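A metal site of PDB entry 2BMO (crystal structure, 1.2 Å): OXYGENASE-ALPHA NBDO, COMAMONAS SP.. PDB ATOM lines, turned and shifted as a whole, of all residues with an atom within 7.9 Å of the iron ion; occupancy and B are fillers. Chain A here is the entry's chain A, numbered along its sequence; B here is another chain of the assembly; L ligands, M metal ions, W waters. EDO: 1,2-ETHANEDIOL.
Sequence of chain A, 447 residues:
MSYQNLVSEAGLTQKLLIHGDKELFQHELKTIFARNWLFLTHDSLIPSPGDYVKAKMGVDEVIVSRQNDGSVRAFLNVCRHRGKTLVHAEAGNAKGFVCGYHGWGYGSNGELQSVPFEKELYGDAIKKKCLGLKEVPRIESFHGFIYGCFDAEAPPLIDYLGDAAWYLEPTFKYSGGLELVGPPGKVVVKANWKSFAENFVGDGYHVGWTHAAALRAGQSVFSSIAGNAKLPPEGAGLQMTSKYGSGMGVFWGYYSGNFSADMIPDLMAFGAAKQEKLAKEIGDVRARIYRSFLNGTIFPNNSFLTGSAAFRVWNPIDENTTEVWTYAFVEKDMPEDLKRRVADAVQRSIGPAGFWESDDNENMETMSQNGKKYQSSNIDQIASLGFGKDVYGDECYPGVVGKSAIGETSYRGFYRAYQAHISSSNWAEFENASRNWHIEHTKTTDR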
ATOM      1  N   ASN A 199      26.230  21.200   0.543  1.00  0.00           N
ATOM      2  CA  ASN A 199      26.828  19.925   0.162  1.00  0.00           C
ATOM      3  C   ASN A 199      27.950  20.136  -0.850  1.00  0.00           C
ATOM      4  O   ASN A 199      29.046  19.570  -0.719  1.00  0.00           O
ATOM      5  CB  ASN A 199      25.754  18.985  -0.383  1.00  0.00           C
ATOM      6  CG  ASN A 199      26.291  17.617  -0.699  1.00  0.00           C
ATOM      7  OD1 ASN A 199      26.485  17.282  -1.852  1.00  0.00           O
ATOM      8  ND2 ASN A 199      26.540  16.800   0.332  1.00  0.00           N
ATOM      9  N   PHE A 200      27.714  20.991  -1.835  1.00  0.00           N
ATOM     10  CA  PHE A 200      28.742  21.247  -2.840  1.00  0.00           C
ATOM     11  C   PHE A 200      29.847  22.187  -2.399  1.00  0.00           C
ATOM     12  O   PHE A 200      30.973  22.068  -2.894  1.00  0.00           O
ATOM     13  CB  PHE A 200      28.128  21.674  -4.178  1.00  0.00           C
ATOM     14  CG  PHE A 200      27.733  20.516  -5.031  1.00  0.00           C
ATOM     15  CD1 PHE A 200      26.643  19.710  -4.687  1.00  0.00           C
ATOM     16  CD2 PHE A 200      28.478  20.173  -6.148  1.00  0.00           C
ATOM     17  CE1 PHE A 200      26.298  18.607  -5.454  1.00  0.00           C
ATOM     18  CE2 PHE A 200      28.136  19.068  -6.929  1.00  0.00           C
ATOM     19  CZ  PHE A 200      27.051  18.283  -6.581  1.00  0.00           C
ATOM     20  N   ASP A 203      31.410  19.575   1.140  1.00  0.00           N
ATOM     21  CA  ASP A 203      31.170  18.240   1.723  1.00  0.00           C
ATOM     22  C   ASP A 203      32.031  17.130   1.113  1.00  0.00           C
ATOM     23  O   ASP A 203      31.545  16.326   0.308  1.00  0.00           O
ATOM     24  CB  ASP A 203      29.683  17.876   1.717  1.00  0.00           C
ATOM     25  CG  ASP A 203      29.356  16.811   2.739  1.00  0.00           C
ATOM     26  OD1 ASP A 203      28.186  16.699   3.131  1.00  0.00           O
ATOM     27  OD2 ASP A 203      30.286  16.095   3.161  1.00  0.00           O
ATOM     28  N   HIS A 206      31.090  13.438   3.134  1.00  0.00           N
ATOM     29  CA  HIS A 206      30.001  12.494   2.813  1.00  0.00           C
ATOM     30  C   HIS A 206      30.408  11.434   1.798  1.00  0.00           C
ATOM     31  O   HIS A 206      29.790  10.365   1.745  1.00  0.00           O
ATOM     32  CB  HIS A 206      28.740  13.220   2.317  1.00  0.00           C
ATOM     33  CG  HIS A 206      28.748  13.535   0.839  1.00  0.00           C
ATOM     34  ND1 HIS A 206      29.519  14.532   0.296  1.00  0.00           N
ATOM     35  CD2 HIS A 206      28.047  13.006  -0.193  1.00  0.00           C
ATOM     36  CE1 HIS A 206      29.316  14.600  -1.003  1.00  0.00           C
ATOM     37  NE2 HIS A 206      28.417  13.686  -1.330  1.00  0.00           N
ATOM     38  N   VAL A 207      31.415  11.721   0.988  1.00  0.00           N
ATOM     39  CA  VAL A 207      31.669  10.931  -0.207  1.00  0.00           C
ATOM     40  C   VAL A 207      31.826   9.446   0.093  1.00  0.00           C
ATOM     41  O   VAL A 207      31.138   8.605  -0.497  1.00  0.00           O
ATOM     42  CB  VAL A 207      32.874  11.463  -1.022  1.00  0.00           C
ATOM     43  CG1 VAL A 207      33.161  10.566  -2.214  1.00  0.00           C
ATOM     44  CG2 VAL A 207      32.617  12.900  -1.473  1.00  0.00           C
ATOM     45  N   GLY A 208      32.696   9.121   1.039  1.00  0.00           N
ATOM     46  CA  GLY A 208      33.006   7.731   1.339  1.00  0.00           C
ATOM     47  C   GLY A 208      31.872   6.956   1.997  1.00  0.00           C
ATOM     48  O   GLY A 208      31.880   5.730   1.981  1.00  0.00           O
ATOM     49  N   THR A 210      28.042   8.213   2.108  1.00  0.00           N
ATOM     50  CA  THR A 210      26.868   8.353   1.256  1.00  0.00           C
ATOM     51  C   THR A 210      27.010   7.547  -0.033  1.00  0.00           C
ATOM     52  O   THR A 210      26.067   6.887  -0.469  1.00  0.00           O
ATOM     53  CB  THR A 210      26.633   9.835   0.923  1.00  0.00           C
ATOM     54  OG1 THR A 210      26.093  10.512   2.065  1.00  0.00           O
ATOM     55  CG2 THR A 210      25.681  10.016  -0.236  1.00  0.00           C
ATOM     56  N   HIS A 211      28.194   7.618  -0.654  1.00  0.00           N
ATOM     57  CA  HIS A 211      28.417   7.009  -1.965  1.00  0.00           C
ATOM     58  C   HIS A 211      29.155   5.679  -1.915  1.00  0.00           C
ATOM     59  O   HIS A 211      29.685   5.235  -2.947  1.00  0.00           O
ATOM     60  CB  HIS A 211      29.137   7.987  -2.905  1.00  0.00           C
ATOM     61  CG  HIS A 211      28.395   9.269  -3.106  1.00  0.00           C
ATOM     62  ND1 HIS A 211      27.159   9.324  -3.720  1.00  0.00           N
ATOM     63  CD2 HIS A 211      28.726  10.546  -2.815  1.00  0.00           C
ATOM     64  CE1 HIS A 211      26.752  10.582  -3.779  1.00  0.00           C
ATOM     65  NE2 HIS A 211      27.679  11.344  -3.225  1.00  0.00           N
ATOM     66  N   ASN A 258      33.944  11.887  -9.907  1.00  0.00           N
ATOM     67  CA  ASN A 258      32.911  10.880  -9.657  1.00  0.00           C
ATOM     68  C   ASN A 258      32.625   9.972 -10.856  1.00  0.00           C
ATOM     69  O   ASN A 258      31.643   9.231 -10.848  1.00  0.00           O
ATOM     70  CB  ASN A 258      31.619  11.524  -9.127  1.00  0.00           C
ATOM     71  CG  ASN A 258      30.965  12.468 -10.127  1.00  0.00           C
ATOM     72  OD1 ASN A 258      31.172  12.370 -11.327  1.00  0.00           O
ATOM     73  ND2 ASN A 258      30.168  13.398  -9.607  1.00  0.00           N
ATOM     74  N   PHE A 293      40.424  17.465  -8.253  1.00  0.00           N
ATOM     75  CA  PHE A 293      38.970  17.567  -8.096  1.00  0.00           C
ATOM     76  C   PHE A 293      38.652  18.703  -7.147  1.00  0.00           C
ATOM     77  O   PHE A 293      39.011  18.655  -5.964  1.00  0.00           O
ATOM     78  CB  PHE A 293      38.436  16.242  -7.561  1.00  0.00           C
ATOM     79  CG  PHE A 293      36.942  16.234  -7.303  1.00  0.00           C
ATOM     80  CD1 PHE A 293      36.061  15.841  -8.300  1.00  0.00           C
ATOM     81  CD2 PHE A 293      36.425  16.584  -6.050  1.00  0.00           C
ATOM     82  CE1 PHE A 293      34.682  15.780  -8.059  1.00  0.00           C
ATOM     83  CE2 PHE A 293      35.048  16.531  -5.803  1.00  0.00           C
ATOM     84  CZ  PHE A 293      34.187  16.130  -6.809  1.00  0.00           C
ATOM     85  N   LEU A 305      31.802  21.035 -10.006  1.00  0.00           N
ATOM     86  CA  LEU A 305      32.894  20.092  -9.810  1.00  0.00           C
ATOM     87  C   LEU A 305      33.859  20.272 -10.971  1.00  0.00           C
ATOM     88  O   LEU A 305      33.433  20.421 -12.109  1.00  0.00           O
ATOM     89  CB  LEU A 305      32.389  18.648  -9.838  1.00  0.00           C
ATOM     90  CG  LEU A 305      31.263  18.275  -8.879  1.00  0.00           C
ATOM     91  CD1 LEU A 305      30.825  16.825  -9.091  1.00  0.00           C
ATOM     92  CD2 LEU A 305      31.634  18.532  -7.436  1.00  0.00           C
ATOM     93  N   ARG A 312      26.323  23.490 -11.943  1.00  0.00           N
ATOM     94  CA  ARG A 312      24.967  23.294 -11.428  1.00  0.00           C
ATOM     95  C   ARG A 312      24.336  24.573 -10.929  1.00  0.00           C
ATOM     96  O   ARG A 312      25.041  25.458 -10.417  1.00  0.00           O
ATOM     97  CB  ARG A 312      24.966  22.271 -10.283  1.00  0.00           C
ATOM     98  CG  ARG A 312      25.589  20.945 -10.651  1.00  0.00           C
ATOM     99  CD  ARG A 312      25.279  19.885  -9.604  1.00  0.00           C
ATOM    100  NE  ARG A 312      24.129  19.056  -9.985  1.00  0.00           N
ATOM    101  CZ  ARG A 312      23.754  17.966  -9.336  1.00  0.00           C
ATOM    102  NH1 ARG A 312      24.419  17.563  -8.269  1.00  0.00           N
ATOM    103  NH2 ARG A 312      22.694  17.275  -9.763  1.00  0.00           N
ATOM    104  N   ILE A 350      25.462  12.497 -11.859  1.00  0.00           N
ATOM    105  CA  ILE A 350      24.724  13.487 -11.079  1.00  0.00           C
ATOM    106  C   ILE A 350      23.567  14.169 -11.784  1.00  0.00           C
ATOM    107  O   ILE A 350      22.993  15.124 -11.234  1.00  0.00           O
ATOM    108  CB  ILE A 350      25.646  14.561 -10.436  1.00  0.00           C
ATOM    109  CG1 ILE A 350      26.425  15.309 -11.514  1.00  0.00           C
ATOM    110  CG2 ILE A 350      26.539  13.908  -9.377  1.00  0.00           C
ATOM    111  CD1 ILE A 350      27.175  16.528 -11.017  1.00  0.00           C
ATOM    112  N   TRP A 356      24.854   8.593  -8.486  1.00  0.00           N
ATOM    113  CA  TRP A 356      25.365   9.302  -7.312  1.00  0.00           C
ATOM    114  C   TRP A 356      24.338  10.309  -6.804  1.00  0.00           C
ATOM    115  O   TRP A 356      24.147  10.433  -5.592  1.00  0.00           O
ATOM    116  CB  TRP A 356      26.653  10.053  -7.615  1.00  0.00           C
ATOM    117  CG  TRP A 356      27.849   9.201  -7.906  1.00  0.00           C
ATOM    118  CD1 TRP A 356      27.968   8.243  -8.874  1.00  0.00           C
ATOM    119  CD2 TRP A 356      29.123   9.293  -7.275  1.00  0.00           C
ATOM    120  NE1 TRP A 356      29.242   7.705  -8.859  1.00  0.00           N
ATOM    121  CE2 TRP A 356      29.971   8.357  -7.895  1.00  0.00           C
ATOM    122  CE3 TRP A 356      29.635  10.096  -6.241  1.00  0.00           C
ATOM    123  CZ2 TRP A 356      31.304   8.184  -7.507  1.00  0.00           C
ATOM    124  CZ3 TRP A 356      30.962   9.931  -5.862  1.00  0.00           C
ATOM    125  CH2 TRP A 356      31.775   8.974  -6.498  1.00  0.00           C
ATOM    126  N   GLU A 357      23.688  11.024  -7.720  1.00  0.00           N
ATOM    127  CA  GLU A 357      22.674  12.007  -7.366  1.00  0.00           C
ATOM    128  C   GLU A 357      21.559  11.408  -6.511  1.00  0.00           C
ATOM    129  O   GLU A 357      21.078  12.043  -5.557  1.00  0.00           O
ATOM    130  CB  GLU A 357      22.085  12.643  -8.636  1.00  0.00           C
ATOM    131  CG  GLU A 357      21.231  13.883  -8.398  1.00  0.00           C
ATOM    132  CD  GLU A 357      22.032  15.123  -8.020  1.00  0.00           C
ATOM    133  OE1 GLU A 357      23.274  15.031  -7.856  1.00  0.00           O
ATOM    134  OE2 GLU A 357      21.416  16.203  -7.876  1.00  0.00           O
ATOM    135  N   ASP A 359      21.952   9.108  -4.333  1.00  0.00           N
ATOM    136  CA  ASP A 359      22.520   9.063  -2.974  1.00  0.00           C
ATOM    137  C   ASP A 359      22.482  10.455  -2.323  1.00  0.00           C
ATOM    138  O   ASP A 359      22.126  10.566  -1.149  1.00  0.00           O
ATOM    139  CB  ASP A 359      23.977   8.611  -2.953  1.00  0.00           C
ATOM    140  CG  ASP A 359      24.241   7.297  -3.676  1.00  0.00           C
ATOM    141  OD1 ASP A 359      25.380   7.181  -4.177  1.00  0.00           O
ATOM    142  OD2 ASP A 359      23.376   6.400  -3.732  1.00  0.00           O
ATOM    143  N   ASP A 360      22.902  11.491  -3.058  1.00  0.00           N
ATOM    144  CA  ASP A 360      22.958  12.850  -2.497  1.00  0.00           C
ATOM    145  C   ASP A 360      21.565  13.362  -2.126  1.00  0.00           C
ATOM    146  O   ASP A 360      21.383  13.944  -1.051  1.00  0.00           O
ATOM    147  CB  ASP A 360      23.643  13.844  -3.451  1.00  0.00           C
ATOM    148  CG  ASP A 360      25.142  13.601  -3.613  1.00  0.00           C
ATOM    149  OD1 ASP A 360      25.932  13.610  -2.643  1.00  0.00           O
ATOM    150  OD2 ASP A 360      25.585  13.437  -4.765  1.00  0.00           O
ATOM    151  N   ASN A 361      20.584  13.148  -3.009  1.00  0.00           N
ATOM    152  CA  ASN A 361      19.211  13.620  -2.788  1.00  0.00           C
ATOM    153  C   ASN A 361      18.561  12.985  -1.564  1.00  0.00           C
ATOM    154  O   ASN A 361      17.709  13.592  -0.909  1.00  0.00           O
ATOM    155  CB  ASN A 361      18.351  13.324  -4.016  1.00  0.00           C
ATOM    156  CG  ASN A 361      18.655  14.244  -5.177  1.00  0.00           C
ATOM    157  OD1 ASN A 361      19.499  15.130  -5.086  1.00  0.00           O
ATOM    158  ND2 ASN A 361      17.944  14.038  -6.281  1.00  0.00           N
ATOM    159  N   ASN A 363      20.006  12.563   1.158  1.00  0.00           N
ATOM    160  CA  ASN A 363      20.402  13.474   2.236  1.00  0.00           C
ATOM    161  C   ASN A 363      19.704  14.847   2.206  1.00  0.00           C
ATOM    162  O   ASN A 363      19.244  15.343   3.225  1.00  0.00           O
ATOM    163  CB  ASN A 363      21.918  13.673   2.187  1.00  0.00           C
ATOM    164  CG  ASN A 363      22.661  12.380   2.369  1.00  0.00           C
ATOM    165  OD1 ASN A 363      22.251  11.535   3.166  1.00  0.00           O
ATOM    166  ND2 ASN A 363      23.746  12.207   1.637  1.00  0.00           N
ATOM    167  N   MET A 364      19.625  15.442   1.022  1.00  0.00           N
ATOM    168  CA  MET A 364      19.053  16.789   0.857  1.00  0.00           C
ATOM    169  C   MET A 364      17.591  16.867   1.279  1.00  0.00           C
ATOM    170  O   MET A 364      17.173  17.809   1.986  1.00  0.00           O
ATOM    171  CB  MET A 364      19.166  17.222  -0.610  1.00  0.00           C
ATOM    172  CG  MET A 364      20.581  17.187  -1.214  1.00  0.00           C
ATOM    173  SD  MET A 364      21.699  18.326  -0.406  1.00  0.00           S
ATOM    174  CE  MET A 364      22.539  17.265   0.766  1.00  0.00           C
ATOM    175  N   TYR B 101      24.403   9.893   6.030  1.00  0.00           N
ATOM    176  CA  TYR B 101      25.035  11.005   5.344  1.00  0.00           C
ATOM    177  C   TYR B 101      26.564  10.914   5.509  1.00  0.00           C
ATOM    178  O   TYR B 101      27.276  10.695   4.517  1.00  0.00           O
ATOM    179  CB  TYR B 101      24.440  12.321   5.871  1.00  0.00           C
ATOM    180  CG  TYR B 101      24.649  13.569   5.008  1.00  0.00           C
ATOM    181  CD1 TYR B 101      23.949  14.733   5.321  1.00  0.00           C
ATOM    182  CD2 TYR B 101      25.532  13.591   3.921  1.00  0.00           C
ATOM    183  CE1 TYR B 101      24.125  15.910   4.575  1.00  0.00           C
ATOM    184  CE2 TYR B 101      25.707  14.760   3.169  1.00  0.00           C
ATOM    185  CZ  TYR B 101      25.010  15.910   3.498  1.00  0.00           C
ATOM    186  OH  TYR B 101      25.179  17.068   2.762  1.00  0.00           O
HETATM  187  C1  EDO L   1      29.160  16.519  -4.247  1.00  0.00           C
HETATM  188  O1  EDO L   1      28.088  15.697  -3.752  1.00  0.00           O
HETATM  189  C2  EDO L   1      29.610  17.502  -3.174  1.00  0.00           C
HETATM  190  O2  EDO L   1      31.024  17.417  -3.013  1.00  0.00           O
HETATM  191 FE    FE M   1      27.764  13.430  -3.259  1.00  0.00          FE
HETATM  192  O   HOH W   1      29.596  13.397  -4.249  1.00  0.00           O
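The iron ion is bound by the side-chain carboxylate (OD1) of Asp 360 (1.9 Å), a ring nitrogen (NE2) of His 206 (2.1 Å), water W1 (2.1 Å), a ring nitrogen (NE2) of His 211 (2.1 Å) and an oxygen (O1) of the ligand (2.3 Å).
The iron ion has five donor atoms within binding distance.
Slightly farther from the iron ion lies OD2 of Asp 360 (2.6 Å).
The nearest printed residue that does not touch the iron ion is Asn 199 (4.3 Å).
A ring nitrogen (ND1) of His 211 is in hydrogen-bond range of the side-chain carboxylate (OD1) of Asp 359.
The backbone carbonyl oxygen (O) of Asp 203 sits at hydrogen-bond distance from a ring nitrogen (ND1) of His 206, 2.7 Å away.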
